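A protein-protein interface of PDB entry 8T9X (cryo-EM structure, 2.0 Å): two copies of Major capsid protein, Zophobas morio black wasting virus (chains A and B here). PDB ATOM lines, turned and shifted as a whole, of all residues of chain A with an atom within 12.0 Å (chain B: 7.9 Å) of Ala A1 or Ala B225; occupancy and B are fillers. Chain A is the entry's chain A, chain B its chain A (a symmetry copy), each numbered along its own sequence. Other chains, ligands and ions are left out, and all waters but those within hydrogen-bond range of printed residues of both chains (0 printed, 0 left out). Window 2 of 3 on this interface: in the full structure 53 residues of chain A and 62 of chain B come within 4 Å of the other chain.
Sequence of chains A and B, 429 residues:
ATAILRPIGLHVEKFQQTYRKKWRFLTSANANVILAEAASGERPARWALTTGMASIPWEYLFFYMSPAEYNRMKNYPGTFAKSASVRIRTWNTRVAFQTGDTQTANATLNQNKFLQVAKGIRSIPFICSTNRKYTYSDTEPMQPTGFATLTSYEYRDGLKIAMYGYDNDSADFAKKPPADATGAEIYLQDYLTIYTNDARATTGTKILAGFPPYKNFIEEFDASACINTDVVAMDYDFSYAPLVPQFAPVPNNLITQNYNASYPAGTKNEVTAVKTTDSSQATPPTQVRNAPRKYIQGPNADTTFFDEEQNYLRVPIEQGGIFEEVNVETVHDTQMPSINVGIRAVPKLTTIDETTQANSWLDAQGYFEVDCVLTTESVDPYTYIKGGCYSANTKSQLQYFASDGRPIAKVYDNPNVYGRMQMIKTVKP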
ATOM      1  N   ALA A   1      16.247  -3.291  13.548  1.00  0.00           N
ATOM      2  CA  ALA A   1      16.414  -4.305  12.514  1.00  0.00           C
ATOM      3  C   ALA A   1      17.266  -5.463  13.019  1.00  0.00           C
ATOM      4  O   ALA A   1      18.232  -5.265  13.754  1.00  0.00           O
ATOM      5  CB  ALA A   1      17.032  -3.697  11.272  1.00  0.00           C
ATOM      6  N   THR A   2      16.894  -6.671  12.612  1.00  0.00           N
ATOM      7  CA  THR A   2      17.609  -7.865  13.035  1.00  0.00           C
ATOM      8  C   THR A   2      19.015  -7.881  12.447  1.00  0.00           C
ATOM      9  O   THR A   2      19.206  -7.642  11.251  1.00  0.00           O
ATOM     10  CB  THR A   2      16.838  -9.108  12.602  1.00  0.00           C
ATOM     11  OG1 THR A   2      17.679 -10.262  12.699  1.00  0.00           O
ATOM     12  CG2 THR A   2      16.368  -8.942  11.175  1.00  0.00           C
ATOM     13  N   ALA A   3      20.000  -8.156  13.293  1.00  0.00           N
ATOM     14  CA  ALA A   3      21.392  -8.198  12.872  1.00  0.00           C
ATOM     15  C   ALA A   3      21.798  -9.644  12.633  1.00  0.00           C
ATOM     16  O   ALA A   3      21.800 -10.454  13.565  1.00  0.00           O
ATOM     17  CB  ALA A   3      22.294  -7.549  13.918  1.00  0.00           C
ATOM     18  N   ILE A   4      22.138  -9.968  11.385  1.00  0.00           N
ATOM     19  CA  ILE A   4      22.631 -11.305  11.080  1.00  0.00           C
ATOM     20  C   ILE A   4      24.109 -11.451  11.426  1.00  0.00           C
ATOM     21  O   ILE A   4      24.568 -12.569  11.689  1.00  0.00           O
ATOM     22  CB  ILE A   4      22.362 -11.653   9.604  1.00  0.00           C
ATOM     23  CG1 ILE A   4      22.615 -13.139   9.343  1.00  0.00           C
ATOM     24  CG2 ILE A   4      23.206 -10.795   8.676  1.00  0.00           C
ATOM     25  CD1 ILE A   4      21.847 -13.693   8.166  1.00  0.00           C
ATOM     26  N   LEU A   5      24.865 -10.356  11.455  1.00  0.00           N
ATOM     27  CA  LEU A   5      26.251 -10.372  11.894  1.00  0.00           C
ATOM     28  C   LEU A   5      26.496  -9.224  12.861  1.00  0.00           C
ATOM     29  O   LEU A   5      25.975  -8.120  12.689  1.00  0.00           O
ATOM     30  CB  LEU A   5      27.231 -10.268  10.716  1.00  0.00           C
ATOM     31  CG  LEU A   5      27.282 -11.418   9.709  1.00  0.00           C
ATOM     32  CD1 LEU A   5      28.087 -11.010   8.485  1.00  0.00           C
ATOM     33  CD2 LEU A   5      27.863 -12.671  10.335  1.00  0.00           C
ATOM     34  N   ARG A   6      27.294  -9.503  13.886  1.00  0.00           N
ATOM     35  CA  ARG A   6      27.749  -8.518  14.851  1.00  0.00           C
ATOM     36  C   ARG A   6      29.255  -8.642  15.016  1.00  0.00           C
ATOM     37  O   ARG A   6      29.819  -9.712  14.770  1.00  0.00           O
ATOM     38  CB  ARG A   6      27.054  -8.702  16.209  1.00  0.00           C
ATOM     39  CG  ARG A   6      25.581  -8.342  16.198  1.00  0.00           C
ATOM     40  CD  ARG A   6      25.204  -7.500  17.413  1.00  0.00           C
ATOM     41  NE  ARG A   6      23.763  -7.323  17.570  1.00  0.00           N
ATOM     42  CZ  ARG A   6      22.891  -8.298  17.792  1.00  0.00           C
ATOM     43  NH1 ARG A   6      23.272  -9.561  17.904  1.00  0.00           N
ATOM     44  NH2 ARG A   6      21.601  -7.998  17.917  1.00  0.00           N
ATOM     45  N   PRO A   7      29.936  -7.565  15.402  1.00  0.00           N
ATOM     46  CA  PRO A   7      31.398  -7.632  15.525  1.00  0.00           C
ATOM     47  C   PRO A   7      31.858  -8.395  16.757  1.00  0.00           C
ATOM     48  O   PRO A   7      32.257  -7.789  17.753  1.00  0.00           O
ATOM     49  CB  PRO A   7      31.814  -6.156  15.602  1.00  0.00           C
ATOM     50  CG  PRO A   7      30.618  -5.382  15.178  1.00  0.00           C
ATOM     51  CD  PRO A   7      29.445  -6.194  15.585  1.00  0.00           C
ATOM     52  N   THR B  90      19.894   5.315   5.668  1.00  0.00           N
ATOM     53  CA  THR B  90      19.672   4.491   4.490  1.00  0.00           C
ATOM     54  C   THR B  90      18.209   4.553   4.073  1.00  0.00           C
ATOM     55  O   THR B  90      17.308   4.616   4.913  1.00  0.00           O
ATOM     56  CB  THR B  90      20.094   3.040   4.734  1.00  0.00           C
ATOM     57  OG1 THR B  90      19.842   2.259   3.561  1.00  0.00           O
ATOM     58  CG2 THR B  90      19.353   2.442   5.897  1.00  0.00           C
ATOM     59  N   ASN B  92      15.353   2.942   0.858  1.00  0.00           N
ATOM     60  CA  ASN B  92      15.019   1.629   0.320  1.00  0.00           C
ATOM     61  C   ASN B  92      16.147   1.099  -0.557  1.00  0.00           C
ATOM     62  O   ASN B  92      16.698   1.820  -1.392  1.00  0.00           O
ATOM     63  CB  ASN B  92      13.719   1.700  -0.484  1.00  0.00           C
ATOM     64  CG  ASN B  92      13.043   0.347  -0.621  1.00  0.00           C
ATOM     65  OD1 ASN B  92      13.493  -0.645  -0.054  1.00  0.00           O
ATOM     66  ND2 ASN B  92      11.965   0.299  -1.392  1.00  0.00           N
ATOM     67  N   LYS B 113      17.830  -9.058   1.557  1.00  0.00           N
ATOM     68  CA  LYS B 113      18.739  -7.926   1.408  1.00  0.00           C
ATOM     69  C   LYS B 113      19.422  -7.647   2.736  1.00  0.00           C
ATOM     70  O   LYS B 113      18.761  -7.612   3.777  1.00  0.00           O
ATOM     71  CB  LYS B 113      17.988  -6.673   0.945  1.00  0.00           C
ATOM     72  CG  LYS B 113      17.250  -6.829  -0.359  1.00  0.00           C
ATOM     73  CD  LYS B 113      16.533  -5.547  -0.740  1.00  0.00           C
ATOM     74  CE  LYS B 113      15.327  -5.283   0.132  1.00  0.00           C
ATOM     75  NZ  LYS B 113      14.433  -4.292  -0.512  1.00  0.00           N
ATOM     76  N   LEU B 115      22.381  -5.102   4.758  1.00  0.00           N
ATOM     77  CA  LEU B 115      23.201  -3.897   4.808  1.00  0.00           C
ATOM     78  C   LEU B 115      24.415  -4.146   5.693  1.00  0.00           C
ATOM     79  O   LEU B 115      24.279  -4.666   6.802  1.00  0.00           O
ATOM     80  CB  LEU B 115      22.387  -2.720   5.346  1.00  0.00           C
ATOM     81  CG  LEU B 115      23.158  -1.563   5.979  1.00  0.00           C
ATOM     82  CD1 LEU B 115      23.787  -0.671   4.925  1.00  0.00           C
ATOM     83  CD2 LEU B 115      22.262  -0.765   6.912  1.00  0.00           C
ATOM     84  N   GLU B 220      26.014  -6.439  10.246  1.00  0.00           N
ATOM     85  CA  GLU B 220      25.171  -6.696   9.089  1.00  0.00           C
ATOM     86  C   GLU B 220      23.721  -6.776   9.536  1.00  0.00           C
ATOM     87  O   GLU B 220      23.394  -7.535  10.450  1.00  0.00           O
ATOM     88  CB  GLU B 220      25.589  -7.983   8.370  1.00  0.00           C
ATOM     89  CG  GLU B 220      24.991  -8.133   6.986  1.00  0.00           C
ATOM     90  CD  GLU B 220      25.682  -9.196   6.156  1.00  0.00           C
ATOM     91  OE1 GLU B 220      26.928  -9.176   6.077  1.00  0.00           O
ATOM     92  OE2 GLU B 220      24.981 -10.047   5.576  1.00  0.00           O
ATOM     93  N   PHE B 221      22.859  -5.995   8.890  1.00  0.00           N
ATOM     94  CA  PHE B 221      21.453  -5.901   9.250  1.00  0.00           C
ATOM     95  C   PHE B 221      20.566  -6.265   8.069  1.00  0.00           C
ATOM     96  O   PHE B 221      20.960  -6.135   6.908  1.00  0.00           O
ATOM     97  CB  PHE B 221      21.078  -4.489   9.724  1.00  0.00           C
ATOM     98  CG  PHE B 221      22.105  -3.841  10.599  1.00  0.00           C
ATOM     99  CD1 PHE B 221      23.057  -2.991  10.064  1.00  0.00           C
ATOM    100  CD2 PHE B 221      22.098  -4.055  11.967  1.00  0.00           C
ATOM    101  CE1 PHE B 221      23.995  -2.387  10.873  1.00  0.00           C
ATOM    102  CE2 PHE B 221      23.031  -3.450  12.783  1.00  0.00           C
ATOM    103  CZ  PHE B 221      23.980  -2.614  12.234  1.00  0.00           C
ATOM    104  N   ASP B 222      19.357  -6.723   8.386  1.00  0.00           N
ATOM    105  CA  ASP B 222      18.305  -6.911   7.397  1.00  0.00           C
ATOM    106  C   ASP B 222      17.965  -5.573   6.750  1.00  0.00           C
ATOM    107  O   ASP B 222      17.455  -4.668   7.415  1.00  0.00           O
ATOM    108  CB  ASP B 222      17.074  -7.533   8.062  1.00  0.00           C
ATOM    109  CG  ASP B 222      15.945  -7.817   7.088  1.00  0.00           C
ATOM    110  OD1 ASP B 222      16.120  -7.628   5.868  1.00  0.00           O
ATOM    111  OD2 ASP B 222      14.870  -8.244   7.555  1.00  0.00           O
ATOM    112  N   ALA B 223      18.248  -5.436   5.453  1.00  0.00           N
ATOM    113  CA  ALA B 223      18.019  -4.165   4.778  1.00  0.00           C
ATOM    114  C   ALA B 223      16.534  -3.889   4.581  1.00  0.00           C
ATOM    115  O   ALA B 223      16.137  -2.729   4.431  1.00  0.00           O
ATOM    116  CB  ALA B 223      18.749  -4.140   3.436  1.00  0.00           C
ATOM    117  N   SER B 224      15.703  -4.932   4.580  1.00  0.00           N
ATOM    118  CA  SER B 224      14.263  -4.732   4.459  1.00  0.00           C
ATOM    119  C   SER B 224      13.690  -4.002   5.665  1.00  0.00           C
ATOM    120  O   SER B 224      12.621  -3.391   5.570  1.00  0.00           O
ATOM    121  CB  SER B 224      13.559  -6.077   4.274  1.00  0.00           C
ATOM    122  OG  SER B 224      14.081  -6.780   3.162  1.00  0.00           O
ATOM    123  N   ALA B 225      14.376  -4.056   6.806  1.00  0.00           N
ATOM    124  CA  ALA B 225      13.893  -3.411   8.020  1.00  0.00           C
ATOM    125  C   ALA B 225      14.638  -2.127   8.360  1.00  0.00           C
ATOM    126  O   ALA B 225      14.356  -1.527   9.401  1.00  0.00           O
ATOM    127  CB  ALA B 225      13.989  -4.376   9.205  1.00  0.00           C
ATOM    128  N   CYS B 226      15.577  -1.697   7.524  1.00  0.00           N
ATOM    129  CA  CYS B 226      16.349  -0.490   7.791  1.00  0.00           C
ATOM    130  C   CYS B 226      15.915   0.704   6.955  1.00  0.00           C
ATOM    131  O   CYS B 226      16.610   1.723   6.964  1.00  0.00           O
ATOM    132  CB  CYS B 226      17.842  -0.751   7.560  1.00  0.00           C
ATOM    133  SG  CYS B 226      18.611  -1.830   8.773  1.00  0.00           S
ATOM    134  N   ILE B 227      14.789   0.620   6.250  1.00  0.00           N
ATOM    135  CA  ILE B 227      14.384   1.703   5.362  1.00  0.00           C
ATOM    136  C   ILE B 227      14.122   2.958   6.182  1.00  0.00           C
ATOM    137  O   ILE B 227      13.359   2.933   7.155  1.00  0.00           O
ATOM    138  CB  ILE B 227      13.154   1.300   4.544  1.00  0.00           C
ATOM    139  CG1 ILE B 227      13.488   0.113   3.640  1.00  0.00           C
ATOM    140  CG2 ILE B 227      12.652   2.473   3.718  1.00  0.00           C
ATOM    141  CD1 ILE B 227      12.288  -0.715   3.261  1.00  0.00           C
ATOM    142  N   ASN B 228      14.771   4.061   5.796  1.00  0.00           N
ATOM    143  CA  ASN B 228      14.567   5.372   6.418  1.00  0.00           C
ATOM    144  C   ASN B 228      14.988   5.365   7.889  1.00  0.00           C
ATOM    145  O   ASN B 228      14.284   5.873   8.764  1.00  0.00           O
ATOM    146  CB  ASN B 228      13.110   5.815   6.266  1.00  0.00           C
ATOM    147  CG  ASN B 228      12.897   7.275   6.599  1.00  0.00           C
ATOM    148  OD1 ASN B 228      13.815   7.986   7.003  1.00  0.00           O
ATOM    149  ND2 ASN B 228      11.656   7.709   6.495  1.00  0.00           N
ATOM    150  N   THR B 229      16.148   4.774   8.167  1.00  0.00           N
ATOM    151  CA  THR B 229      16.682   4.695   9.520  1.00  0.00           C
ATOM    152  C   THR B 229      18.150   5.098   9.536  1.00  0.00           C
ATOM    153  O   THR B 229      18.874   4.907   8.556  1.00  0.00           O
ATOM    154  CB  THR B 229      16.537   3.277  10.121  1.00  0.00           C
ATOM    155  OG1 THR B 229      17.427   2.374   9.451  1.00  0.00           O
ATOM    156  CG2 THR B 229      15.109   2.765   9.999  1.00  0.00           C
ATOM    157  N   VAL B 231      21.936   4.559  10.472  1.00  0.00           N
ATOM    158  CA  VAL B 231      22.754   3.365  10.644  1.00  0.00           C
ATOM    159  C   VAL B 231      24.118   3.729  11.218  1.00  0.00           C
ATOM    160  O   VAL B 231      24.754   2.907  11.885  1.00  0.00           O
ATOM    161  CB  VAL B 231      22.895   2.588   9.321  1.00  0.00           C
ATOM    162  CG1 VAL B 231      21.526   2.222   8.783  1.00  0.00           C
ATOM    163  CG2 VAL B 231      23.675   3.390   8.297  1.00  0.00           C
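The backbone carbonyl oxygen (O) of Thr A2 is in hydrogen-bond range of the backbone NH (N) of Asp B222. The backbone NH of Ile A4 lies within hydrogen-bond range of the backbone carbonyl oxygen of Glu B220, 2.9 Å away. The backbone NH (N) of Glu B220 lies within hydrogen-bond range of the backbone carbonyl oxygen (O) of Leu A5, 3.0 Å away.
N of Leu B115 lies within hydrogen-bond range of O of Phe B221 (2.8 Å). The backbone NH (N) of Ser B224 sits at hydrogen-bond distance from the side-chain carboxylate (OD1) of Asp B222, at 3.0 Å. SG of Cys B226 lies within hydrogen-bond range of O of Asp B222. O of Cys B226 lies within hydrogen-bond range of OG1 of Thr B229 (2.7 Å).
Among the printed residues, merely in contact across the chains: Ala A1 with Asp B222, Ala A1 with Ala B225, Ala A1 with Cys B226, Thr A2 with Phe B221 and Ala A3 with Glu B220.
Of the printed residues of chain B, Ala A1 touches Asp B222, Ala B225 and Cys B226. Of the printed residues of chain A, Ala B225 touches Ala A1 (3.7 Å). No residue of chain A comes within 4 Å of Ser B224. No residue of chain A comes within 4 Å of Ile B227. Of the printed residues of chain B, Thr A2 touches Phe B221 and Asp B222. Of the printed residues of chain A, Asp B222 touches Ala A1 and Thr A2. Of the printed residues of chain B, Ala A3 touches Glu B220 (3.2 Å). Arg A6 touches none of the printed residues of chain B. Thr B90 touches none of the printed residues of chain A. The nearest printed residue of chain B that does not touch Ala A1 is Phe B221 (4.4 Å). The nearest residue of chain A that does not touch Ala B225 is Thr A2 (5.0 Å). The nearest printed residue of chain B that does not touch Thr A2 is Glu B220 (4.3 Å).
Hydrophobic or aromatic side chains of chain A within 4 Å of the printed part of chain B: Ala A1, Ala A3, Ile A4 and Leu A5. Printed residues of chain B that touch a printed residue of chain A: Glu B220, Phe B221, Asp B222, Ala B225 and Cys B226. Hydrophobic or aromatic side chains of chain B within 4 Å of the printed part of chain A: Phe B221 and Ala B225.
No position is printed for both chains.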
